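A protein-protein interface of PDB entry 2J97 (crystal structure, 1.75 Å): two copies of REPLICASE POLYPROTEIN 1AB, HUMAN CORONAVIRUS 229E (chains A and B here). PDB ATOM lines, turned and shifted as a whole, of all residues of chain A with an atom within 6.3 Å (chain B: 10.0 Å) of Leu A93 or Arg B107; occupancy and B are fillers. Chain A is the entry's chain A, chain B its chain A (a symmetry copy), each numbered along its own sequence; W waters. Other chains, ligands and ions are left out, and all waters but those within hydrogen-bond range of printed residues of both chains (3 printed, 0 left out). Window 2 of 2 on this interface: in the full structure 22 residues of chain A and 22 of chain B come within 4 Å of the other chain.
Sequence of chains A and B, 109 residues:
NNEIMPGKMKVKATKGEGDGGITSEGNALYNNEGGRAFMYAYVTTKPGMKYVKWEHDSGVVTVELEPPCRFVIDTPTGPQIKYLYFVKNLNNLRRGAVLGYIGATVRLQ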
ATOM      1  N   ASN A  91      -3.254  -6.866  15.763  1.00  0.00           N
ATOM      2  CA  ASN A  91      -4.368  -6.891  14.801  1.00  0.00           C
ATOM      3  C   ASN A  91      -4.667  -8.305  14.316  1.00  0.00           C
ATOM      4  O   ASN A  91      -3.915  -9.222  14.637  1.00  0.00           O
ATOM      5  CB  ASN A  91      -4.170  -5.888  13.646  1.00  0.00           C
ATOM      6  CG  ASN A  91      -3.114  -6.312  12.646  1.00  0.00           C
ATOM      7  OD1 ASN A  91      -2.584  -7.431  12.664  1.00  0.00           O
ATOM      8  ND2 ASN A  91      -2.825  -5.402  11.714  1.00  0.00           N
ATOM      9  N   ASN A  92      -5.776  -8.486  13.592  1.00  0.00           N
ATOM     10  CA  ASN A  92      -6.243  -9.836  13.244  1.00  0.00           C
ATOM     11  C   ASN A  92      -5.311 -10.506  12.243  1.00  0.00           C
ATOM     12  O   ASN A  92      -5.153 -11.715  12.260  1.00  0.00           O
ATOM     13  CB  ASN A  92      -7.670  -9.794  12.683  1.00  0.00           C
ATOM     14  CG  ASN A  92      -8.677  -9.583  13.759  1.00  0.00           C
ATOM     15  OD1 ASN A  92      -8.362  -9.764  14.955  1.00  0.00           O
ATOM     16  ND2 ASN A  92      -9.901  -9.168  13.373  1.00  0.00           N
ATOM     17  N   LEU A  93      -4.673  -9.710  11.385  1.00  0.00           N
ATOM     18  CA  LEU A  93      -3.753 -10.266  10.393  1.00  0.00           C
ATOM     19  C   LEU A  93      -2.626 -11.009  11.117  1.00  0.00           C
ATOM     20  O   LEU A  93      -2.307 -12.168  10.787  1.00  0.00           O
ATOM     21  CB  LEU A  93      -3.191  -9.129   9.528  1.00  0.00           C
ATOM     22  CG  LEU A  93      -2.347  -9.497   8.320  1.00  0.00           C
ATOM     23  CD1 LEU A  93      -3.256 -10.157   7.234  1.00  0.00           C
ATOM     24  CD2 LEU A  93      -1.667  -8.185   7.810  1.00  0.00           C
ATOM     25  N   ARG A  94      -2.100 -10.362  12.149  1.00  0.00           N
ATOM     26  CA  ARG A  94      -0.993 -10.907  12.926  1.00  0.00           C
ATOM     27  C   ARG A  94      -1.449 -11.965  13.905  1.00  0.00           C
ATOM     28  O   ARG A  94      -0.757 -12.977  14.093  1.00  0.00           O
ATOM     29  CB  ARG A  94      -0.266  -9.778  13.646  1.00  0.00           C
ATOM     30  CG  ARG A  94       0.502  -8.870  12.645  1.00  0.00           C
ATOM     31  CD  ARG A  94       1.093  -7.649  13.323  1.00  0.00           C
ATOM     32  NE  ARG A  94       1.807  -6.837  12.330  1.00  0.00           N
ATOM     33  CZ  ARG A  94       1.331  -5.724  11.786  1.00  0.00           C
ATOM     34  NH1 ARG A  94       0.132  -5.267  12.137  1.00  0.00           N
ATOM     35  NH2 ARG A  94       2.059  -5.049  10.890  1.00  0.00           N
ATOM     36  N   ARG A  95      -2.600 -11.762  14.542  1.00  0.00           N
ATOM     37  CA  ARG A  95      -3.177 -12.880  15.335  1.00  0.00           C
ATOM     38  C   ARG A  95      -3.302 -14.165  14.499  1.00  0.00           C
ATOM     39  O   ARG A  95      -2.980 -15.276  14.972  1.00  0.00           O
ATOM     40  CB  ARG A  95      -4.560 -12.517  15.916  1.00  0.00           C
ATOM     41  CG  ARG A  95      -4.539 -11.431  16.964  1.00  0.00           C
ATOM     42  CD  ARG A  95      -6.011 -10.946  17.288  1.00  0.00           C
ATOM     43  NE  ARG A  95      -5.821  -9.756  18.079  1.00  0.00           N
ATOM     44  CZ  ARG A  95      -5.659  -9.718  19.402  1.00  0.00           C
ATOM     45  NH1 ARG A  95      -5.844 -10.808  20.152  1.00  0.00           N
ATOM     46  NH2 ARG A  95      -5.357  -8.558  19.972  1.00  0.00           N
ATOM     47  N   GLY A  96      -3.787 -14.027  13.263  1.00  0.00           N
ATOM     48  CA  GLY A  96      -3.972 -15.206  12.410  1.00  0.00           C
ATOM     49  C   GLY A  96      -2.639 -15.850  12.024  1.00  0.00           C
ATOM     50  O   GLY A  96      -2.526 -17.090  11.964  1.00  0.00           O
ATOM     51  N   ALA A  97      -1.644 -15.011  11.760  1.00  0.00           N
ATOM     52  CA  ALA A  97      -0.309 -15.510  11.406  1.00  0.00           C
ATOM     53  C   ALA A  97       0.270 -16.305  12.568  1.00  0.00           C
ATOM     54  O   ALA A  97       0.912 -17.335  12.349  1.00  0.00           O
ATOM     55  CB  ALA A  97       0.616 -14.370  11.083  1.00  0.00           C
ATOM     56  N   VAL A  98       0.061 -15.796  13.784  1.00  0.00           N
ATOM     57  CA  VAL A  98       0.560 -16.481  14.990  1.00  0.00           C
ATOM     58  C   VAL A  98      -0.108 -17.835  15.137  1.00  0.00           C
ATOM     59  O   VAL A  98       0.567 -18.842  15.359  1.00  0.00           O
ATOM     60  CB  VAL A  98       0.330 -15.631  16.260  1.00  0.00           C
ATOM     61  CG1 VAL A  98       0.548 -16.473  17.519  1.00  0.00           C
ATOM     62  CG2 VAL A  98       1.287 -14.404  16.254  1.00  0.00           C
ATOM     63  N   PHE B  71      -9.337 -16.522  23.360  1.00  0.00           N
ATOM     64  CA  PHE B  71      -8.513 -15.655  22.514  1.00  0.00           C
ATOM     65  C   PHE B  71      -9.380 -14.537  22.010  1.00  0.00           C
ATOM     66  O   PHE B  71     -10.529 -14.756  21.662  1.00  0.00           O
ATOM     67  CB  PHE B  71      -7.858 -16.405  21.325  1.00  0.00           C
ATOM     68  CG  PHE B  71      -8.828 -17.004  20.332  1.00  0.00           C
ATOM     69  CD1 PHE B  71      -9.013 -16.425  19.072  1.00  0.00           C
ATOM     70  CD2 PHE B  71      -9.528 -18.186  20.622  1.00  0.00           C
ATOM     71  CE1 PHE B  71      -9.880 -16.988  18.159  1.00  0.00           C
ATOM     72  CE2 PHE B  71     -10.411 -18.765  19.700  1.00  0.00           C
ATOM     73  CZ  PHE B  71     -10.596 -18.151  18.454  1.00  0.00           C
ATOM     74  N   VAL B  72      -8.797 -13.345  21.997  1.00  0.00           N
ATOM     75  CA  VAL B  72      -9.436 -12.144  21.462  1.00  0.00           C
ATOM     76  C   VAL B  72      -9.271 -12.037  19.956  1.00  0.00           C
ATOM     77  O   VAL B  72      -8.223 -12.366  19.396  1.00  0.00           O
ATOM     78  CB  VAL B  72      -8.866 -10.911  22.147  1.00  0.00           C
ATOM     79  CG1 VAL B  72      -9.166  -9.604  21.373  1.00  0.00           C
ATOM     80  CG2 VAL B  72      -9.429 -10.836  23.587  1.00  0.00           C
ATOM     81  N   ILE B  73     -10.342 -11.613  19.292  1.00  0.00           N
ATOM     82  CA  ILE B  73     -10.205 -11.144  17.927  1.00  0.00           C
ATOM     83  C   ILE B  73     -10.746  -9.713  17.876  1.00  0.00           C
ATOM     84  O   ILE B  73     -11.653  -9.348  18.651  1.00  0.00           O
ATOM     85  CB  ILE B  73     -10.923 -12.070  16.921  1.00  0.00           C
ATOM     86  CG1 ILE B  73     -12.430 -12.024  17.050  1.00  0.00           C
ATOM     87  CG2 ILE B  73     -10.430 -13.502  17.069  1.00  0.00           C
ATOM     88  CD1 ILE B  73     -13.171 -12.561  15.799  1.00  0.00           C
ATOM     89  N   ASP B  74     -10.173  -8.903  16.994  1.00  0.00           N
ATOM     90  CA  ASP B  74     -10.708  -7.567  16.761  1.00  0.00           C
ATOM     91  C   ASP B  74     -12.013  -7.670  15.963  1.00  0.00           C
ATOM     92  O   ASP B  74     -12.188  -8.554  15.102  1.00  0.00           O
ATOM     93  CB  ASP B  74      -9.697  -6.714  15.980  1.00  0.00           C
ATOM     94  CG  ASP B  74      -8.529  -6.257  16.825  1.00  0.00           C
ATOM     95  OD1 ASP B  74      -8.601  -6.365  18.079  1.00  0.00           O
ATOM     96  OD2 ASP B  74      -7.547  -5.753  16.207  1.00  0.00           O
ATOM     97  N   LEU B  99      -5.740 -25.118  14.572  1.00  0.00           N
ATOM     98  CA  LEU B  99      -5.118 -23.807  14.781  1.00  0.00           C
ATOM     99  C   LEU B  99      -4.843 -23.054  13.448  1.00  0.00           C
ATOM    100  O   LEU B  99      -5.041 -21.841  13.367  1.00  0.00           O
ATOM    101  CB  LEU B  99      -3.816 -23.948  15.558  1.00  0.00           C
ATOM    102  CG  LEU B  99      -4.057 -24.325  17.039  1.00  0.00           C
ATOM    103  CD1 LEU B  99      -2.769 -24.812  17.719  1.00  0.00           C
ATOM    104  CD2 LEU B  99      -4.732 -23.186  17.845  1.00  0.00           C
ATOM    105  N   GLY B 100      -4.349 -23.774  12.457  1.00  0.00           N
ATOM    106  CA  GLY B 100      -4.113 -23.215  11.132  1.00  0.00           C
ATOM    107  C   GLY B 100      -5.403 -22.722  10.480  1.00  0.00           C
ATOM    108  O   GLY B 100      -5.418 -21.634   9.898  1.00  0.00           O
ATOM    109  N   TYR B 101      -6.476 -23.502  10.589  1.00  0.00           N
ATOM    110  CA  TYR B 101      -7.773 -23.111  10.022  1.00  0.00           C
ATOM    111  C   TYR B 101      -8.301 -21.842  10.700  1.00  0.00           C
ATOM    112  O   TYR B 101      -8.758 -20.906  10.027  1.00  0.00           O
ATOM    113  CB  TYR B 101      -8.788 -24.251  10.121  1.00  0.00           C
ATOM    114  CG  TYR B 101     -10.094 -23.929   9.414  1.00  0.00           C
ATOM    115  CD1 TYR B 101     -10.314 -24.353   8.106  1.00  0.00           C
ATOM    116  CD2 TYR B 101     -11.098 -23.187  10.042  1.00  0.00           C
ATOM    117  CE1 TYR B 101     -11.493 -24.045   7.441  1.00  0.00           C
ATOM    118  CE2 TYR B 101     -12.297 -22.889   9.377  1.00  0.00           C
ATOM    119  CZ  TYR B 101     -12.473 -23.323   8.086  1.00  0.00           C
ATOM    120  OH  TYR B 101     -13.638 -23.030   7.399  1.00  0.00           O
ATOM    121  N   ILE B 102      -8.217 -21.789  12.020  1.00  0.00           N
ATOM    122  CA  ILE B 102      -8.661 -20.601  12.745  1.00  0.00           C
ATOM    123  C   ILE B 102      -7.790 -19.403  12.396  1.00  0.00           C
ATOM    124  O   ILE B 102      -8.294 -18.311  12.173  1.00  0.00           O
ATOM    125  CB  ILE B 102      -8.702 -20.854  14.259  1.00  0.00           C
ATOM    126  CG1 ILE B 102      -9.757 -21.927  14.550  1.00  0.00           C
ATOM    127  CG2 ILE B 102      -8.945 -19.542  15.046  1.00  0.00           C
ATOM    128  CD1 ILE B 102      -9.797 -22.407  15.974  1.00  0.00           C
ATOM    129  N   GLY B 103      -6.482 -19.619  12.305  1.00  0.00           N
ATOM    130  CA  GLY B 103      -5.579 -18.545  11.893  1.00  0.00           C
ATOM    131  C   GLY B 103      -5.998 -17.999  10.528  1.00  0.00           C
ATOM    132  O   GLY B 103      -6.042 -16.782  10.343  1.00  0.00           O
ATOM    133  N   ALA B 104      -6.317 -18.906   9.606  1.00  0.00           N
ATOM    134  CA  ALA B 104      -6.667 -18.524   8.212  1.00  0.00           C
ATOM    135  C   ALA B 104      -7.950 -17.700   8.166  1.00  0.00           C
ATOM    136  O   ALA B 104      -8.082 -16.778   7.324  1.00  0.00           O
ATOM    137  CB  ALA B 104      -6.816 -19.769   7.346  1.00  0.00           C
ATOM    138  N   THR B 105      -8.890 -18.033   9.055  1.00  0.00           N
ATOM    139  CA  THR B 105     -10.172 -17.310   9.149  1.00  0.00           C
ATOM    140  C   THR B 105      -9.984 -15.954   9.851  1.00  0.00           C
ATOM    141  O   THR B 105     -10.447 -14.908   9.381  1.00  0.00           O
ATOM    142  CB  THR B 105     -11.227 -18.161   9.883  1.00  0.00           C
ATOM    143  OG1 THR B 105     -11.351 -19.435   9.216  1.00  0.00           O
ATOM    144  CG2 THR B 105     -12.599 -17.462   9.852  1.00  0.00           C
ATOM    145  N   VAL B 106      -9.299 -15.963  10.985  1.00  0.00           N
ATOM    146  CA  VAL B 106      -9.091 -14.725  11.747  1.00  0.00           C
ATOM    147  C   VAL B 106      -8.343 -13.643  10.939  1.00  0.00           C
ATOM    148  O   VAL B 106      -8.708 -12.466  10.977  1.00  0.00           O
ATOM    149  CB  VAL B 106      -8.339 -15.040  13.071  1.00  0.00           C
ATOM    150  CG1 VAL B 106      -7.841 -13.747  13.732  1.00  0.00           C
ATOM    151  CG2 VAL B 106      -9.229 -15.860  14.010  1.00  0.00           C
ATOM    152  N   ARG B 107      -7.328 -14.027  10.164  1.00  0.00           N
ATOM    153  CA  ARG B 107      -6.554 -13.005   9.434  1.00  0.00           C
ATOM    154  C   ARG B 107      -7.398 -12.196   8.416  1.00  0.00           C
ATOM    155  O   ARG B 107      -6.999 -11.114   7.998  1.00  0.00           O
ATOM    156  CB  ARG B 107      -5.352 -13.639   8.746  1.00  0.00           C
ATOM    157  CG  ARG B 107      -5.711 -14.683   7.701  1.00  0.00           C
ATOM    158  CD  ARG B 107      -4.462 -15.273   7.077  1.00  0.00           C
ATOM    159  NE  ARG B 107      -3.714 -14.213   6.408  1.00  0.00           N
ATOM    160  CZ  ARG B 107      -3.916 -13.836   5.139  1.00  0.00           C
ATOM    161  NH1 ARG B 107      -4.816 -14.454   4.373  1.00  0.00           N
ATOM    162  NH2 ARG B 107      -3.203 -12.840   4.629  1.00  0.00           N
ATOM    163  N   LEU B 108      -8.541 -12.738   8.008  1.00  0.00           N
ATOM    164  CA  LEU B 108      -9.390 -12.089   6.980  1.00  0.00           C
ATOM    165  C   LEU B 108     -10.372 -11.066   7.551  1.00  0.00           C
ATOM    166  O   LEU B 108     -10.955 -10.259   6.810  1.00  0.00           O
ATOM    167  CB  LEU B 108     -10.170 -13.166   6.184  1.00  0.00           C
ATOM    168  CG  LEU B 108      -9.276 -14.108   5.360  1.00  0.00           C
ATOM    169  CD1 LEU B 108     -10.157 -15.119   4.594  1.00  0.00           C
ATOM    170  CD2 LEU B 108      -8.345 -13.365   4.376  1.00  0.00           C
ATOM    171  N   GLN B 109     -10.577 -11.074   8.858  1.00  0.00           N
ATOM    172  CA  GLN B 109     -11.661 -10.246   9.369  1.00  0.00           C
ATOM    173  C   GLN B 109     -11.259  -9.104  10.262  1.00  0.00           C
ATOM    174  O   GLN B 109     -10.089  -8.785  10.380  1.00  0.00           O
ATOM    175  CB  GLN B 109     -12.765 -11.084   9.973  1.00  0.00           C
ATOM    176  CG  GLN B 109     -12.310 -12.095  11.000  1.00  0.00           C
ATOM    177  CD  GLN B 109     -13.319 -13.217  11.106  1.00  0.00           C
ATOM    178  OE1 GLN B 109     -13.922 -13.405  12.168  1.00  0.00           O
ATOM    179  NE2 GLN B 109     -13.545 -13.950   9.985  1.00  0.00           N
ATOM    180  OXT GLN B 109     -12.143  -8.454  10.822  1.00  0.00           O
HETATM  181  O   HOH W   1      -7.597  -6.192  13.302  1.00  0.00           O
HETATM  182  O   HOH W   2      -6.709  -5.499  19.555  1.00  0.00           O
HETATM  183  O   HOH W   3      -1.717 -13.242   8.314  1.00  0.00           O
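Of the 8 printed residues of chain A, 5 touch a printed residue of chain B. Hydrophobic or aromatic side chains of chain A within 4 Å of the printed part of chain B: Leu A93. Among the printed residues, 9 pairs touch across the chains.
Among the printed residues, merely in contact across the chains: Asn A91 with Asp B74 (3.7 Å), Asn A92 with Ile B73 (3.8 Å), Asn A92 with Val B106 (3.3 Å), Asn A92 with Arg B107 (3.4 Å), Leu A93 with Arg B107 (3.7 Å) and Gly A96 with Gly B103 (3.3 Å).
The side-chain amide nitrogen (ND2) of Asn A92 is in hydrogen-bond range of the chain-end carboxylate (O) of Gln B109, 3.0 Å away. The side-chain amide oxygen (OD1) of Asn A92 lies within hydrogen-bond range of the backbone NH (N) of Asp B74 (2.9 Å). The guanidinium group (NH1) of Arg A95 sits at hydrogen-bond distance from the backbone carbonyl oxygen (O) of Val B72 (2.9 Å).
Of the printed residues of chain B, Leu A93 touches Arg B107 (3.7 Å). Arg B107 touches just these residues of chain A: Asn A92 and Leu A93. Of chain B, only Asp B74 (3.7 Å) comes within 4 Å of Asn A91. Asn A92 touches just these residues of chain B: Ile B73, Asp B74, Val B106, Arg B107 and Gln B109. No residue of chain B comes within 4 Å of Arg A94. Printed residues of chain A within 4 Å of Gln B109: Asn A92. Printed residues of chain A within 4 Å of Val B106: Asn A92. Printed residues of chain A within 4 Å of Gly B103: Gly A96 (3.3 Å). Of the printed residues of chain A, Ile B73 touches Asn A92. Ile B102 touches none of the printed residues of chain A. The nearest residue of chain B that does not touch Leu A93 is Val B106 (4.9 Å). The nearest residue of chain A that does not touch Arg B107 is Gly A96 (4.2 Å). The nearest printed residue of chain A that does not touch Ile B73 is Arg A95 (4.2 Å).
No position is printed for both chains.
ND2 of Asn A91 sits close to NH1 of Arg A94 (3.0 Å). NE2 of Gln B109 lies within hydrogen-bond range of O of Thr B105, at 3.3 Å. N of Leu A93 sits close to OD1 of Asn A91.
Water W2 lies within hydrogen-bond range of the side-chain carboxylate (OD1) of Asp B74 (2.6 Å) and the guanidinium group (NH2) of Arg A95 (3.4 Å). Water W3 lies within hydrogen-bond range of O of Leu A93 (2.8 Å) and NE of Arg B107 (2.9 Å). Water W1 bridges the side-chain carboxylate of Asp B74 (2.9 Å) and the backbone NH of Asn A92 (2.9 Å).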
